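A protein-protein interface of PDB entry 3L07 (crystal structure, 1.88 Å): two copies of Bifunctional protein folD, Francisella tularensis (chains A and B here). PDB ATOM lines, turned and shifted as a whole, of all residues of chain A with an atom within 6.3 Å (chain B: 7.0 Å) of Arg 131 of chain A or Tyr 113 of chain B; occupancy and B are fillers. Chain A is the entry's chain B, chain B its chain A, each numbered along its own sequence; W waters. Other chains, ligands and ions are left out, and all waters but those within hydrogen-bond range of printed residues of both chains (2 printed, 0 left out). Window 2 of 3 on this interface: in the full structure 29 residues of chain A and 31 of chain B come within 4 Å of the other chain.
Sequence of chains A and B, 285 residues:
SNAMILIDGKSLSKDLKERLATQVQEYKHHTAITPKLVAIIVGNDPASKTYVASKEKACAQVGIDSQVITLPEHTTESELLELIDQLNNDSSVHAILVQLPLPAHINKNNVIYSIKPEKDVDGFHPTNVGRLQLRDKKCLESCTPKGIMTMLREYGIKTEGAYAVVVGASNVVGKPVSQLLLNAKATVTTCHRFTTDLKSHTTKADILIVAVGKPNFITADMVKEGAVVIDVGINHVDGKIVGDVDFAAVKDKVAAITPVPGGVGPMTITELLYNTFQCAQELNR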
ATOM      1  N   PRO A 117      19.437 -27.260  26.071  1.00  0.00           N
ATOM      2  CA  PRO A 117      20.847 -27.048  25.744  1.00  0.00           C
ATOM      3  C   PRO A 117      21.418 -25.819  26.445  1.00  0.00           C
ATOM      4  O   PRO A 117      22.600 -25.788  26.748  1.00  0.00           O
ATOM      5  CB  PRO A 117      20.819 -26.831  24.219  1.00  0.00           C
ATOM      6  CG  PRO A 117      19.711 -27.803  23.782  1.00  0.00           C
ATOM      7  CD  PRO A 117      18.638 -27.615  24.880  1.00  0.00           C
ATOM      8  N   GLU A 118      20.577 -24.812  26.668  1.00  0.00           N
ATOM      9  CA  GLU A 118      21.008 -23.553  27.266  1.00  0.00           C
ATOM     10  C   GLU A 118      21.391 -23.701  28.743  1.00  0.00           C
ATOM     11  O   GLU A 118      22.034 -22.811  29.259  1.00  0.00           O
ATOM     12  CB  GLU A 118      19.913 -22.480  27.135  1.00  0.00           C
ATOM     13  CG  GLU A 118      19.600 -22.096  25.718  1.00  0.00           C
ATOM     14  CD  GLU A 118      18.863 -23.199  24.897  1.00  0.00           C
ATOM     15  OE1 GLU A 118      18.178 -24.084  25.493  1.00  0.00           O
ATOM     16  OE2 GLU A 118      18.985 -23.139  23.645  1.00  0.00           O
ATOM     17  N   PRO A 126      23.621 -33.191  22.513  1.00  0.00           N
ATOM     18  CA  PRO A 126      23.943 -33.180  21.088  1.00  0.00           C
ATOM     19  C   PRO A 126      23.954 -31.803  20.418  1.00  0.00           C
ATOM     20  O   PRO A 126      24.800 -31.543  19.571  1.00  0.00           O
ATOM     21  CB  PRO A 126      22.806 -34.042  20.478  1.00  0.00           C
ATOM     22  CG  PRO A 126      22.326 -34.850  21.532  1.00  0.00           C
ATOM     23  CD  PRO A 126      22.650 -34.242  22.840  1.00  0.00           C
ATOM     24  N   THR A 127      23.043 -30.908  20.784  1.00  0.00           N
ATOM     25  CA  THR A 127      23.060 -29.560  20.200  1.00  0.00           C
ATOM     26  C   THR A 127      24.333 -28.788  20.554  1.00  0.00           C
ATOM     27  O   THR A 127      24.835 -28.055  19.715  1.00  0.00           O
ATOM     28  CB  THR A 127      21.778 -28.770  20.594  1.00  0.00           C
ATOM     29  OG1 THR A 127      20.657 -29.299  19.893  1.00  0.00           O
ATOM     30  CG2 THR A 127      21.852 -27.231  20.340  1.00  0.00           C
ATOM     31  N   ASN A 128      24.836 -28.921  21.789  1.00  0.00           N
ATOM     32  CA  ASN A 128      26.084 -28.293  22.157  1.00  0.00           C
ATOM     33  C   ASN A 128      27.273 -28.964  21.430  1.00  0.00           C
ATOM     34  O   ASN A 128      28.161 -28.265  20.894  1.00  0.00           O
ATOM     35  CB  ASN A 128      26.248 -28.251  23.660  1.00  0.00           C
ATOM     36  CG  ASN A 128      25.366 -27.156  24.276  1.00  0.00           C
ATOM     37  OD1 ASN A 128      25.320 -26.059  23.753  1.00  0.00           O
ATOM     38  ND2 ASN A 128      24.637 -27.474  25.315  1.00  0.00           N
ATOM     39  N   VAL A 129      27.252 -30.286  21.354  1.00  0.00           N
ATOM     40  CA  VAL A 129      28.314 -31.038  20.622  1.00  0.00           C
ATOM     41  C   VAL A 129      28.347 -30.552  19.178  1.00  0.00           C
ATOM     42  O   VAL A 129      29.449 -30.252  18.615  1.00  0.00           O
ATOM     43  CB  VAL A 129      28.139 -32.590  20.764  1.00  0.00           C
ATOM     44  CG1 VAL A 129      29.203 -33.376  19.898  1.00  0.00           C
ATOM     45  CG2 VAL A 129      28.291 -33.022  22.270  1.00  0.00           C
ATOM     46  N   GLY A 130      27.170 -30.425  18.580  1.00  0.00           N
ATOM     47  CA  GLY A 130      27.047 -29.977  17.181  1.00  0.00           C
ATOM     48  C   GLY A 130      27.436 -28.508  16.977  1.00  0.00           C
ATOM     49  O   GLY A 130      28.171 -28.160  16.031  1.00  0.00           O
ATOM     50  N   ARG A 131      26.971 -27.645  17.869  1.00  0.00           N
ATOM     51  CA  ARG A 131      27.326 -26.231  17.805  1.00  0.00           C
ATOM     52  C   ARG A 131      28.824 -25.994  17.967  1.00  0.00           C
ATOM     53  O   ARG A 131      29.318 -25.046  17.360  1.00  0.00           O
ATOM     54  CB  ARG A 131      26.556 -25.393  18.792  1.00  0.00           C
ATOM     55  CG  ARG A 131      25.152 -25.120  18.338  1.00  0.00           C
ATOM     56  CD  ARG A 131      24.295 -24.538  19.425  1.00  0.00           C
ATOM     57  NE  ARG A 131      23.070 -24.012  18.827  1.00  0.00           N
ATOM     58  CZ  ARG A 131      21.995 -23.636  19.507  1.00  0.00           C
ATOM     59  NH1 ARG A 131      20.971 -23.121  18.819  1.00  0.00           N
ATOM     60  NH2 ARG A 131      21.925 -23.770  20.831  1.00  0.00           N
ATOM     61  N   LEU A 132      29.506 -26.828  18.745  1.00  0.00           N
ATOM     62  CA  LEU A 132      30.964 -26.779  18.866  1.00  0.00           C
ATOM     63  C   LEU A 132      31.583 -26.947  17.469  1.00  0.00           C
ATOM     64  O   LEU A 132      32.329 -26.100  17.020  1.00  0.00           O
ATOM     65  CB  LEU A 132      31.483 -27.833  19.834  1.00  0.00           C
ATOM     66  CG  LEU A 132      32.953 -27.695  20.221  1.00  0.00           C
ATOM     67  CD1 LEU A 132      33.188 -28.263  21.655  1.00  0.00           C
ATOM     68  CD2 LEU A 132      33.847 -28.350  19.249  1.00  0.00           C
ATOM     69  N   GLN A 133      31.201 -28.020  16.796  1.00  0.00           N
ATOM     70  CA  GLN A 133      31.767 -28.403  15.480  1.00  0.00           C
ATOM     71  C   GLN A 133      31.389 -27.296  14.513  1.00  0.00           C
ATOM     72  O   GLN A 133      32.242 -26.761  13.828  1.00  0.00           O
ATOM     73  CB  GLN A 133      31.256 -29.805  15.088  1.00  0.00           C
ATOM     74  CG  GLN A 133      31.504 -30.279  13.637  1.00  0.00           C
ATOM     75  CD  GLN A 133      31.188 -31.718  13.436  1.00  0.00           C
ATOM     76  OE1 GLN A 133      31.235 -32.492  14.400  1.00  0.00           O
ATOM     77  NE2 GLN A 133      30.870 -32.118  12.210  1.00  0.00           N
ATOM     78  N   LEU A 134      30.131 -26.858  14.542  1.00  0.00           N
ATOM     79  CA  LEU A 134      29.622 -25.830  13.634  1.00  0.00           C
ATOM     80  C   LEU A 134      30.036 -24.393  14.009  1.00  0.00           C
ATOM     81  O   LEU A 134      29.483 -23.412  13.478  1.00  0.00           O
ATOM     82  CB  LEU A 134      28.084 -25.907  13.559  1.00  0.00           C
ATOM     83  CG  LEU A 134      27.388 -27.192  13.063  1.00  0.00           C
ATOM     84  CD1 LEU A 134      25.942 -27.197  13.595  1.00  0.00           C
ATOM     85  CD2 LEU A 134      27.385 -27.301  11.522  1.00  0.00           C
ATOM     86  N   ARG A 135      30.952 -24.242  14.959  1.00  0.00           N
ATOM     87  CA  ARG A 135      31.416 -22.894  15.318  1.00  0.00           C
ATOM     88  C   ARG A 135      30.240 -21.946  15.483  1.00  0.00           C
ATOM     89  O   ARG A 135      30.106 -20.983  14.734  1.00  0.00           O
ATOM     90  CB  ARG A 135      32.354 -22.378  14.226  1.00  0.00           C
ATOM     91  CG  ARG A 135      33.809 -22.266  14.658  1.00  0.00           C
ATOM     92  CD  ARG A 135      34.662 -21.822  13.499  1.00  0.00           C
ATOM     93  NE  ARG A 135      34.672 -22.859  12.462  1.00  0.00           N
ATOM     94  CZ  ARG A 135      35.583 -22.969  11.496  1.00  0.00           C
ATOM     95  NH1 ARG A 135      35.504 -23.978  10.637  1.00  0.00           N
ATOM     96  NH2 ARG A 135      36.589 -22.101  11.394  1.00  0.00           N
ATOM     97  N   ASP A 136      29.382 -22.252  16.459  1.00  0.00           N
ATOM     98  CA  ASP A 136      28.191 -21.469  16.811  1.00  0.00           C
ATOM     99  C   ASP A 136      28.391 -21.023  18.263  1.00  0.00           C
ATOM    100  O   ASP A 136      29.042 -21.743  19.036  1.00  0.00           O
ATOM    101  CB  ASP A 136      26.961 -22.375  16.688  1.00  0.00           C
ATOM    102  CG  ASP A 136      25.624 -21.621  16.808  1.00  0.00           C
ATOM    103  OD1 ASP A 136      25.470 -20.715  17.673  1.00  0.00           O
ATOM    104  OD2 ASP A 136      24.711 -22.002  16.030  1.00  0.00           O
ATOM    105  N   LYS A 137      27.815 -19.883  18.659  1.00  0.00           N
ATOM    106  CA  LYS A 137      28.335 -19.169  19.837  1.00  0.00           C
ATOM    107  C   LYS A 137      27.541 -19.402  21.112  1.00  0.00           C
ATOM    108  O   LYS A 137      27.958 -19.013  22.221  1.00  0.00           O
ATOM    109  CB  LYS A 137      28.513 -17.665  19.543  1.00  0.00           C
ATOM    110  CG  LYS A 137      27.360 -16.944  18.750  1.00  0.00           C
ATOM    111  CD  LYS A 137      27.551 -17.057  17.224  1.00  0.00           C
ATOM    112  CE  LYS A 137      26.627 -16.105  16.464  1.00  0.00           C
ATOM    113  NZ  LYS A 137      25.232 -16.032  17.019  1.00  0.00           N
ATOM    114  N   LYS A 138      26.408 -20.071  20.955  1.00  0.00           N
ATOM    115  CA  LYS A 138      25.585 -20.457  22.094  1.00  0.00           C
ATOM    116  C   LYS A 138      26.111 -21.748  22.747  1.00  0.00           C
ATOM    117  O   LYS A 138      25.479 -22.319  23.698  1.00  0.00           O
ATOM    118  CB  LYS A 138      24.126 -20.663  21.652  1.00  0.00           C
ATOM    119  CG  LYS A 138      23.359 -19.372  21.320  1.00  0.00           C
ATOM    120  CD  LYS A 138      22.632 -19.486  19.966  1.00  0.00           C
ATOM    121  CE  LYS A 138      21.272 -18.798  19.980  1.00  0.00           C
ATOM    122  NZ  LYS A 138      20.664 -18.718  18.590  1.00  0.00           N
ATOM    123  N   CYS A 139      27.251 -22.205  22.237  1.00  0.00           N
ATOM    124  CA  CYS A 139      27.669 -23.527  22.510  1.00  0.00           C
ATOM    125  C   CYS A 139      28.186 -23.474  23.959  1.00  0.00           C
ATOM    126  O   CYS A 139      28.967 -22.618  24.315  1.00  0.00           O
ATOM    127  CB  CYS A 139      28.758 -23.924  21.507  1.00  0.00           C
ATOM    128  SG  CYS A 139      29.624 -25.240  21.973  1.00  0.00           S
ATOM    129  N   LEU A 140      27.688 -24.363  24.788  1.00  0.00           N
ATOM    130  CA  LEU A 140      28.381 -24.733  26.017  1.00  0.00           C
ATOM    131  C   LEU A 140      29.368 -25.806  25.566  1.00  0.00           C
ATOM    132  O   LEU A 140      28.983 -26.820  25.057  1.00  0.00           O
ATOM    133  CB  LEU A 140      27.423 -25.235  27.077  1.00  0.00           C
ATOM    134  CG  LEU A 140      26.635 -24.012  27.616  1.00  0.00           C
ATOM    135  CD1 LEU A 140      25.336 -24.295  28.197  1.00  0.00           C
ATOM    136  CD2 LEU A 140      27.641 -23.329  28.633  1.00  0.00           C
ATOM    137  N   ASN A 183      38.928 -25.750  14.873  1.00  0.00           N
ATOM    138  CA  ASN A 183      38.361 -24.386  14.835  1.00  0.00           C
ATOM    139  C   ASN A 183      39.441 -23.345  15.082  1.00  0.00           C
ATOM    140  O   ASN A 183      39.377 -22.242  14.547  1.00  0.00           O
ATOM    141  CB  ASN A 183      37.225 -24.216  15.859  1.00  0.00           C
ATOM    142  CG  ASN A 183      36.006 -25.052  15.497  1.00  0.00           C
ATOM    143  OD1 ASN A 183      35.932 -25.515  14.395  1.00  0.00           O
ATOM    144  ND2 ASN A 183      35.047 -25.207  16.428  1.00  0.00           N
ATOM    145  N   ILE B  84       7.564 -24.398   9.014  1.00  0.00           N
ATOM    146  CA  ILE B  84       8.397 -25.541   9.479  1.00  0.00           C
ATOM    147  C   ILE B  84       7.759 -26.117  10.749  1.00  0.00           C
ATOM    148  O   ILE B  84       7.638 -27.319  10.920  1.00  0.00           O
ATOM    149  CB  ILE B  84       9.892 -25.155   9.644  1.00  0.00           C
ATOM    150  CG1 ILE B  84      10.500 -24.981   8.237  1.00  0.00           C
ATOM    151  CG2 ILE B  84      10.647 -26.224  10.452  1.00  0.00           C
ATOM    152  CD1 ILE B  84      11.951 -24.410   8.194  1.00  0.00           C
ATOM    153  N   ASN B  88       6.705 -29.934  11.372  1.00  0.00           N
ATOM    154  CA  ASN B  88       7.245 -30.683  12.525  1.00  0.00           C
ATOM    155  C   ASN B  88       6.201 -31.486  13.260  1.00  0.00           C
ATOM    156  O   ASN B  88       6.447 -32.611  13.711  1.00  0.00           O
ATOM    157  CB  ASN B  88       7.891 -29.733  13.518  1.00  0.00           C
ATOM    158  CG  ASN B  88       9.244 -29.294  13.076  1.00  0.00           C
ATOM    159  OD1 ASN B  88       9.907 -29.998  12.267  1.00  0.00           O
ATOM    160  ND2 ASN B  88       9.673 -28.101  13.547  1.00  0.00           N
ATOM    161  N   LYS B 108      19.890 -18.997   7.299  1.00  0.00           N
ATOM    162  CA  LYS B 108      19.863 -20.459   7.116  1.00  0.00           C
ATOM    163  C   LYS B 108      19.977 -21.234   8.428  1.00  0.00           C
ATOM    164  O   LYS B 108      19.277 -22.203   8.664  1.00  0.00           O
ATOM    165  CB  LYS B 108      20.994 -20.844   6.151  1.00  0.00           C
ATOM    166  CG  LYS B 108      21.499 -22.252   6.244  1.00  0.00           C
ATOM    167  CD  LYS B 108      22.542 -22.563   5.152  1.00  0.00           C
ATOM    168  CE  LYS B 108      23.923 -22.020   5.418  1.00  0.00           C
ATOM    169  NZ  LYS B 108      24.498 -22.415   6.752  1.00  0.00           N
ATOM    170  N   ASN B 109      20.867 -20.795   9.302  1.00  0.00           N
ATOM    171  CA  ASN B 109      21.089 -21.518  10.532  1.00  0.00           C
ATOM    172  C   ASN B 109      19.857 -21.505  11.420  1.00  0.00           C
ATOM    173  O   ASN B 109      19.551 -22.488  12.072  1.00  0.00           O
ATOM    174  CB  ASN B 109      22.330 -20.979  11.291  1.00  0.00           C
ATOM    175  CG  ASN B 109      23.635 -21.166  10.497  1.00  0.00           C
ATOM    176  OD1 ASN B 109      23.770 -22.072   9.669  1.00  0.00           O
ATOM    177  ND2 ASN B 109      24.585 -20.272  10.734  1.00  0.00           N
ATOM    178  N   ASN B 110      19.131 -20.402  11.451  1.00  0.00           N
ATOM    179  CA  ASN B 110      17.921 -20.351  12.254  1.00  0.00           C
ATOM    180  C   ASN B 110      16.827 -21.274  11.666  1.00  0.00           C
ATOM    181  O   ASN B 110      16.023 -21.872  12.391  1.00  0.00           O
ATOM    182  CB  ASN B 110      17.381 -18.925  12.292  1.00  0.00           C
ATOM    183  CG  ASN B 110      18.217 -18.011  13.117  1.00  0.00           C
ATOM    184  OD1 ASN B 110      19.115 -18.470  13.838  1.00  0.00           O
ATOM    185  ND2 ASN B 110      17.921 -16.691  13.038  1.00  0.00           N
ATOM    186  N   VAL B 111      16.803 -21.341  10.343  1.00  0.00           N
ATOM    187  CA  VAL B 111      15.847 -22.191   9.624  1.00  0.00           C
ATOM    188  C   VAL B 111      16.194 -23.653   9.954  1.00  0.00           C
ATOM    189  O   VAL B 111      15.346 -24.398  10.421  1.00  0.00           O
ATOM    190  CB  VAL B 111      15.920 -21.909   8.143  1.00  0.00           C
ATOM    191  CG1 VAL B 111      15.140 -22.947   7.317  1.00  0.00           C
ATOM    192  CG2 VAL B 111      15.346 -20.485   7.852  1.00  0.00           C
ATOM    193  N   ILE B 112      17.463 -24.015   9.800  1.00  0.00           N
ATOM    194  CA  ILE B 112      17.893 -25.406  10.070  1.00  0.00           C
ATOM    195  C   ILE B 112      17.539 -25.777  11.514  1.00  0.00           C
ATOM    196  O   ILE B 112      16.872 -26.784  11.749  1.00  0.00           O
ATOM    197  CB  ILE B 112      19.366 -25.631   9.800  1.00  0.00           C
ATOM    198  CG1 ILE B 112      19.653 -25.565   8.299  1.00  0.00           C
ATOM    199  CG2 ILE B 112      19.833 -26.980  10.502  1.00  0.00           C
ATOM    200  CD1 ILE B 112      21.147 -25.396   7.892  1.00  0.00           C
ATOM    201  N   TYR B 113      17.865 -24.917  12.475  1.00  0.00           N
ATOM    202  CA  TYR B 113      17.587 -25.219  13.887  1.00  0.00           C
ATOM    203  C   TYR B 113      16.141 -25.461  14.177  1.00  0.00           C
ATOM    204  O   TYR B 113      15.791 -26.228  15.086  1.00  0.00           O
ATOM    205  CB  TYR B 113      18.128 -24.117  14.859  1.00  0.00           C
ATOM    206  CG  TYR B 113      18.183 -24.551  16.331  1.00  0.00           C
ATOM    207  CD1 TYR B 113      19.084 -25.511  16.756  1.00  0.00           C
ATOM    208  CD2 TYR B 113      17.347 -23.977  17.288  1.00  0.00           C
ATOM    209  CE1 TYR B 113      19.140 -25.916  18.106  1.00  0.00           C
ATOM    210  CE2 TYR B 113      17.381 -24.375  18.626  1.00  0.00           C
ATOM    211  CZ  TYR B 113      18.273 -25.341  19.032  1.00  0.00           C
ATOM    212  OH  TYR B 113      18.313 -25.710  20.353  1.00  0.00           O
ATOM    213  N   SER B 114      15.266 -24.802  13.437  1.00  0.00           N
ATOM    214  CA  SER B 114      13.835 -24.928  13.685  1.00  0.00           C
ATOM    215  C   SER B 114      13.211 -26.244  13.230  1.00  0.00           C
ATOM    216  O   SER B 114      12.131 -26.590  13.675  1.00  0.00           O
ATOM    217  CB  SER B 114      13.079 -23.772  13.032  1.00  0.00           C
ATOM    218  OG  SER B 114      13.002 -23.922  11.608  1.00  0.00           O
ATOM    219  N   ILE B 115      13.912 -26.991  12.382  1.00  0.00           N
ATOM    220  CA  ILE B 115      13.446 -28.326  11.979  1.00  0.00           C
ATOM    221  C   ILE B 115      13.597 -29.288  13.123  1.00  0.00           C
ATOM    222  O   ILE B 115      14.644 -29.313  13.765  1.00  0.00           O
ATOM    223  CB  ILE B 115      14.234 -28.809  10.737  1.00  0.00           C
ATOM    224  CG1 ILE B 115      14.135 -27.816   9.591  1.00  0.00           C
ATOM    225  CG2 ILE B 115      13.655 -30.187  10.182  1.00  0.00           C
ATOM    226  CD1 ILE B 115      14.982 -28.152   8.343  1.00  0.00           C
ATOM    227  N   LYS B 116      12.604 -30.121  13.393  1.00  0.00           N
ATOM    228  CA  LYS B 116      12.778 -31.231  14.344  1.00  0.00           C
ATOM    229  C   LYS B 116      13.927 -32.112  13.903  1.00  0.00           C
ATOM    230  O   LYS B 116      13.935 -32.552  12.740  1.00  0.00           O
ATOM    231  CB  LYS B 116      11.503 -32.077  14.371  1.00  0.00           C
ATOM    232  CG  LYS B 116      11.449 -33.186  15.362  1.00  0.00           C
ATOM    233  CD  LYS B 116       9.946 -33.537  15.626  1.00  0.00           C
ATOM    234  CE  LYS B 116       9.759 -34.423  16.877  1.00  0.00           C
ATOM    235  NZ  LYS B 116      10.907 -35.322  17.153  1.00  0.00           N
ATOM    236  N   PRO B 117      14.896 -32.396  14.814  1.00  0.00           N
ATOM    237  CA  PRO B 117      16.068 -33.193  14.373  1.00  0.00           C
ATOM    238  C   PRO B 117      15.692 -34.554  13.791  1.00  0.00           C
ATOM    239  O   PRO B 117      16.256 -34.985  12.815  1.00  0.00           O
ATOM    240  CB  PRO B 117      16.851 -33.390  15.688  1.00  0.00           C
ATOM    241  CG  PRO B 117      16.508 -32.229  16.488  1.00  0.00           C
ATOM    242  CD  PRO B 117      15.078 -31.907  16.200  1.00  0.00           C
ATOM    243  N   PHE B 124      21.931 -31.400   9.075  1.00  0.00           N
ATOM    244  CA  PHE B 124      22.747 -30.296   9.546  1.00  0.00           C
ATOM    245  C   PHE B 124      22.212 -29.635  10.785  1.00  0.00           C
ATOM    246  O   PHE B 124      22.869 -28.769  11.254  1.00  0.00           O
ATOM    247  CB  PHE B 124      23.024 -29.234   8.472  1.00  0.00           C
ATOM    248  CG  PHE B 124      23.734 -29.784   7.235  1.00  0.00           C
ATOM    249  CD1 PHE B 124      25.035 -30.271   7.331  1.00  0.00           C
ATOM    250  CD2 PHE B 124      23.091 -29.842   6.028  1.00  0.00           C
ATOM    251  CE1 PHE B 124      25.697 -30.819   6.190  1.00  0.00           C
ATOM    252  CE2 PHE B 124      23.748 -30.348   4.892  1.00  0.00           C
ATOM    253  CZ  PHE B 124      25.026 -30.856   4.993  1.00  0.00           C
ATOM    254  N   HIS B 125      21.061 -30.036  11.325  1.00  0.00           N
ATOM    255  CA  HIS B 125      20.687 -29.595  12.646  1.00  0.00           C
ATOM    256  C   HIS B 125      21.820 -29.942  13.635  1.00  0.00           C
ATOM    257  O   HIS B 125      22.400 -31.016  13.586  1.00  0.00           O
ATOM    258  CB  HIS B 125      19.426 -30.267  13.115  1.00  0.00           C
ATOM    259  CG  HIS B 125      18.788 -29.618  14.313  1.00  0.00           C
ATOM    260  ND1 HIS B 125      19.316 -29.683  15.589  1.00  0.00           N
ATOM    261  CD2 HIS B 125      17.653 -28.885  14.418  1.00  0.00           C
ATOM    262  CE1 HIS B 125      18.522 -29.043  16.431  1.00  0.00           C
ATOM    263  NE2 HIS B 125      17.496 -28.553  15.748  1.00  0.00           N
ATOM    264  N   PRO B 126      22.147 -29.001  14.531  1.00  0.00           N
ATOM    265  CA  PRO B 126      23.138 -29.298  15.563  1.00  0.00           C
ATOM    266  C   PRO B 126      22.970 -30.595  16.311  1.00  0.00           C
ATOM    267  O   PRO B 126      23.977 -31.265  16.554  1.00  0.00           O
ATOM    268  CB  PRO B 126      23.072 -28.076  16.496  1.00  0.00           C
ATOM    269  CG  PRO B 126      22.504 -26.986  15.641  1.00  0.00           C
ATOM    270  CD  PRO B 126      21.588 -27.646  14.655  1.00  0.00           C
ATOM    271  N   THR B 127      21.746 -30.996  16.644  1.00  0.00           N
ATOM    272  CA  THR B 127      21.523 -32.298  17.289  1.00  0.00           C
ATOM    273  C   THR B 127      21.953 -33.464  16.418  1.00  0.00           C
ATOM    274  O   THR B 127      22.479 -34.425  16.933  1.00  0.00           O
ATOM    275  CB  THR B 127      20.060 -32.457  17.729  1.00  0.00           C
ATOM    276  OG1 THR B 127      19.859 -31.650  18.907  1.00  0.00           O
ATOM    277  CG2 THR B 127      19.718 -33.913  18.071  1.00  0.00           C
ATOM    278  N   VAL B 129      24.305 -33.196  13.971  1.00  0.00           N
ATOM    279  CA  VAL B 129      25.741 -33.103  13.962  1.00  0.00           C
ATOM    280  C   VAL B 129      26.358 -33.744  15.253  1.00  0.00           C
ATOM    281  O   VAL B 129      27.309 -34.527  15.156  1.00  0.00           O
ATOM    282  CB  VAL B 129      26.239 -31.642  13.741  1.00  0.00           C
ATOM    283  CG1 VAL B 129      27.787 -31.565  13.678  1.00  0.00           C
ATOM    284  CG2 VAL B 129      25.698 -31.049  12.438  1.00  0.00           C
ATOM    285  N   GLY B 130      25.821 -33.435  16.422  1.00  0.00           N
ATOM    286  CA  GLY B 130      26.334 -33.980  17.663  1.00  0.00           C
ATOM    287  C   GLY B 130      26.087 -35.486  17.742  1.00  0.00           C
ATOM    288  O   GLY B 130      26.978 -36.259  18.141  1.00  0.00           O
HETATM  289  O   HOH W   1      29.767 -34.706  13.973  1.00  0.00           O
HETATM  290  O   HOH W   2      18.287 -28.385  20.447  1.00  0.00           O
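OG1 of Thr 127 of chain B is in hydrogen-bond range of OG1 of Thr 127 of chain A.
The backbone carbonyl oxygen (O) of Pro 126 of chain A sits close to the backbone carbonyl oxygen (O) of Pro 126 of chain B, at 3.1 Å.
Hydrophobic or aromatic side chains of chain B within 4 Å of the printed part of chain A: Tyr 113, Pro 126 and Val 129.
Along chain B the printed residues that touch a printed residue of chain A span positions 113 to 130.
Of the 18 printed residues of chain A, 6 touch a printed residue of chain B.
Along chain A the printed residues that touch a printed residue of chain B span positions 126 to 133.
Among the printed residues, 12 pairs touch across the chains.
Among the printed residues, no Asp or Glu carboxylate lies within 4 Å of a Lys or Arg side-chain nitrogen of the other chain.
Water W2 lies within hydrogen-bond range of OG1 of Thr 127 of chain A (2.6 Å) and OH of Tyr 113 of chain B (2.7 Å).
Water W1 bridges OE1 of Gln 133 of chain A (2.7 Å) and O of Val 129 of chain B (2.7 Å).
Pro 126 of chain A touches Thr 127 of chain B, and with the chains exchanged Thr 127 of chain A touches Pro 126 of chain B.
Thr 127 of chain B touches its own counterpart, Thr 127 of chain A.
Val 129 of chain A touches Gly 130 of chain B, and with the chains exchanged Gly 130 of chain A touches Val 129 of chain B.
Gly 130 of chain A touches its own counterpart, Gly 130 of chain B.
Of chain B, only Tyr 113 comes within 4 Å of Arg 131 of chain A.
Of chain A, only Thr 127 (3.8 Å) and Arg 131 (3.4 Å) come within 4 Å of Tyr 113 of chain B.
Gly 130 of chain A touches just these residues of chain B: Pro 126 (3.4 Å), Val 129 (3.9 Å) and Gly 130 (3.7 Å).
Of the printed residues of chain B, Pro 126 of chain A touches Pro 126, Thr 127 and Gly 130.
Of the printed residues of chain B, Gln 133 of chain A touches Val 129 (3.4 Å).
The nearest residue of chain B that does not touch Arg 131 of chain A is Pro 126 of chain B (4.1 Å).
The nearest printed residue of chain A that does not touch Tyr 113 of chain B is Glu 118 of chain A (4.2 Å).
The nearest printed residue of chain A that does not touch Val 129 of chain B is Leu 134 of chain A (4.03 Å).
CB of Pro 126 of chain A touches O of Thr 127 of chain B (3.6 Å).
Pro 126 of chain A touches Gly 130 of chain B (O to CA, 3.5 Å).
Thr 127 of chain A touches Tyr 113 of chain B (CG2 to CE1, 3.8 Å).
Pro 126 of chain B touches Thr 127 of chain A.
Val 129 of chain A touches Gly 130 of chain B (CG1 to CA, 3.7 Å).
Gly 130 of chain A touches Pro 126 of chain B.
Gly 130 of chain A touches Val 129 of chain B.
N of Gly 130 of chain B touches CA of Gly 130 of chain A, 3.7 Å away.
Arg 131 of chain A touches Tyr 113 of chain B (NH1 to CE1, 3.4 Å).
CD of Gln 133 of chain A touches CG1 of Val 129 of chain B (3.4 Å).
The backbone carbonyl oxygen (O) of Tyr 113 of chain B is in hydrogen-bond range of a ring nitrogen (NE2) of His 125 of chain B.
ND1 of His 125 of chain B lies within hydrogen-bond range of N of Thr 127 of chain B (3.0 Å).
The guanidinium group (NE) of Arg 131 of chain A lies within salt-bridge range of the side-chain carboxylate (OD2) of Asp 136 of chain A (3.8 Å).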
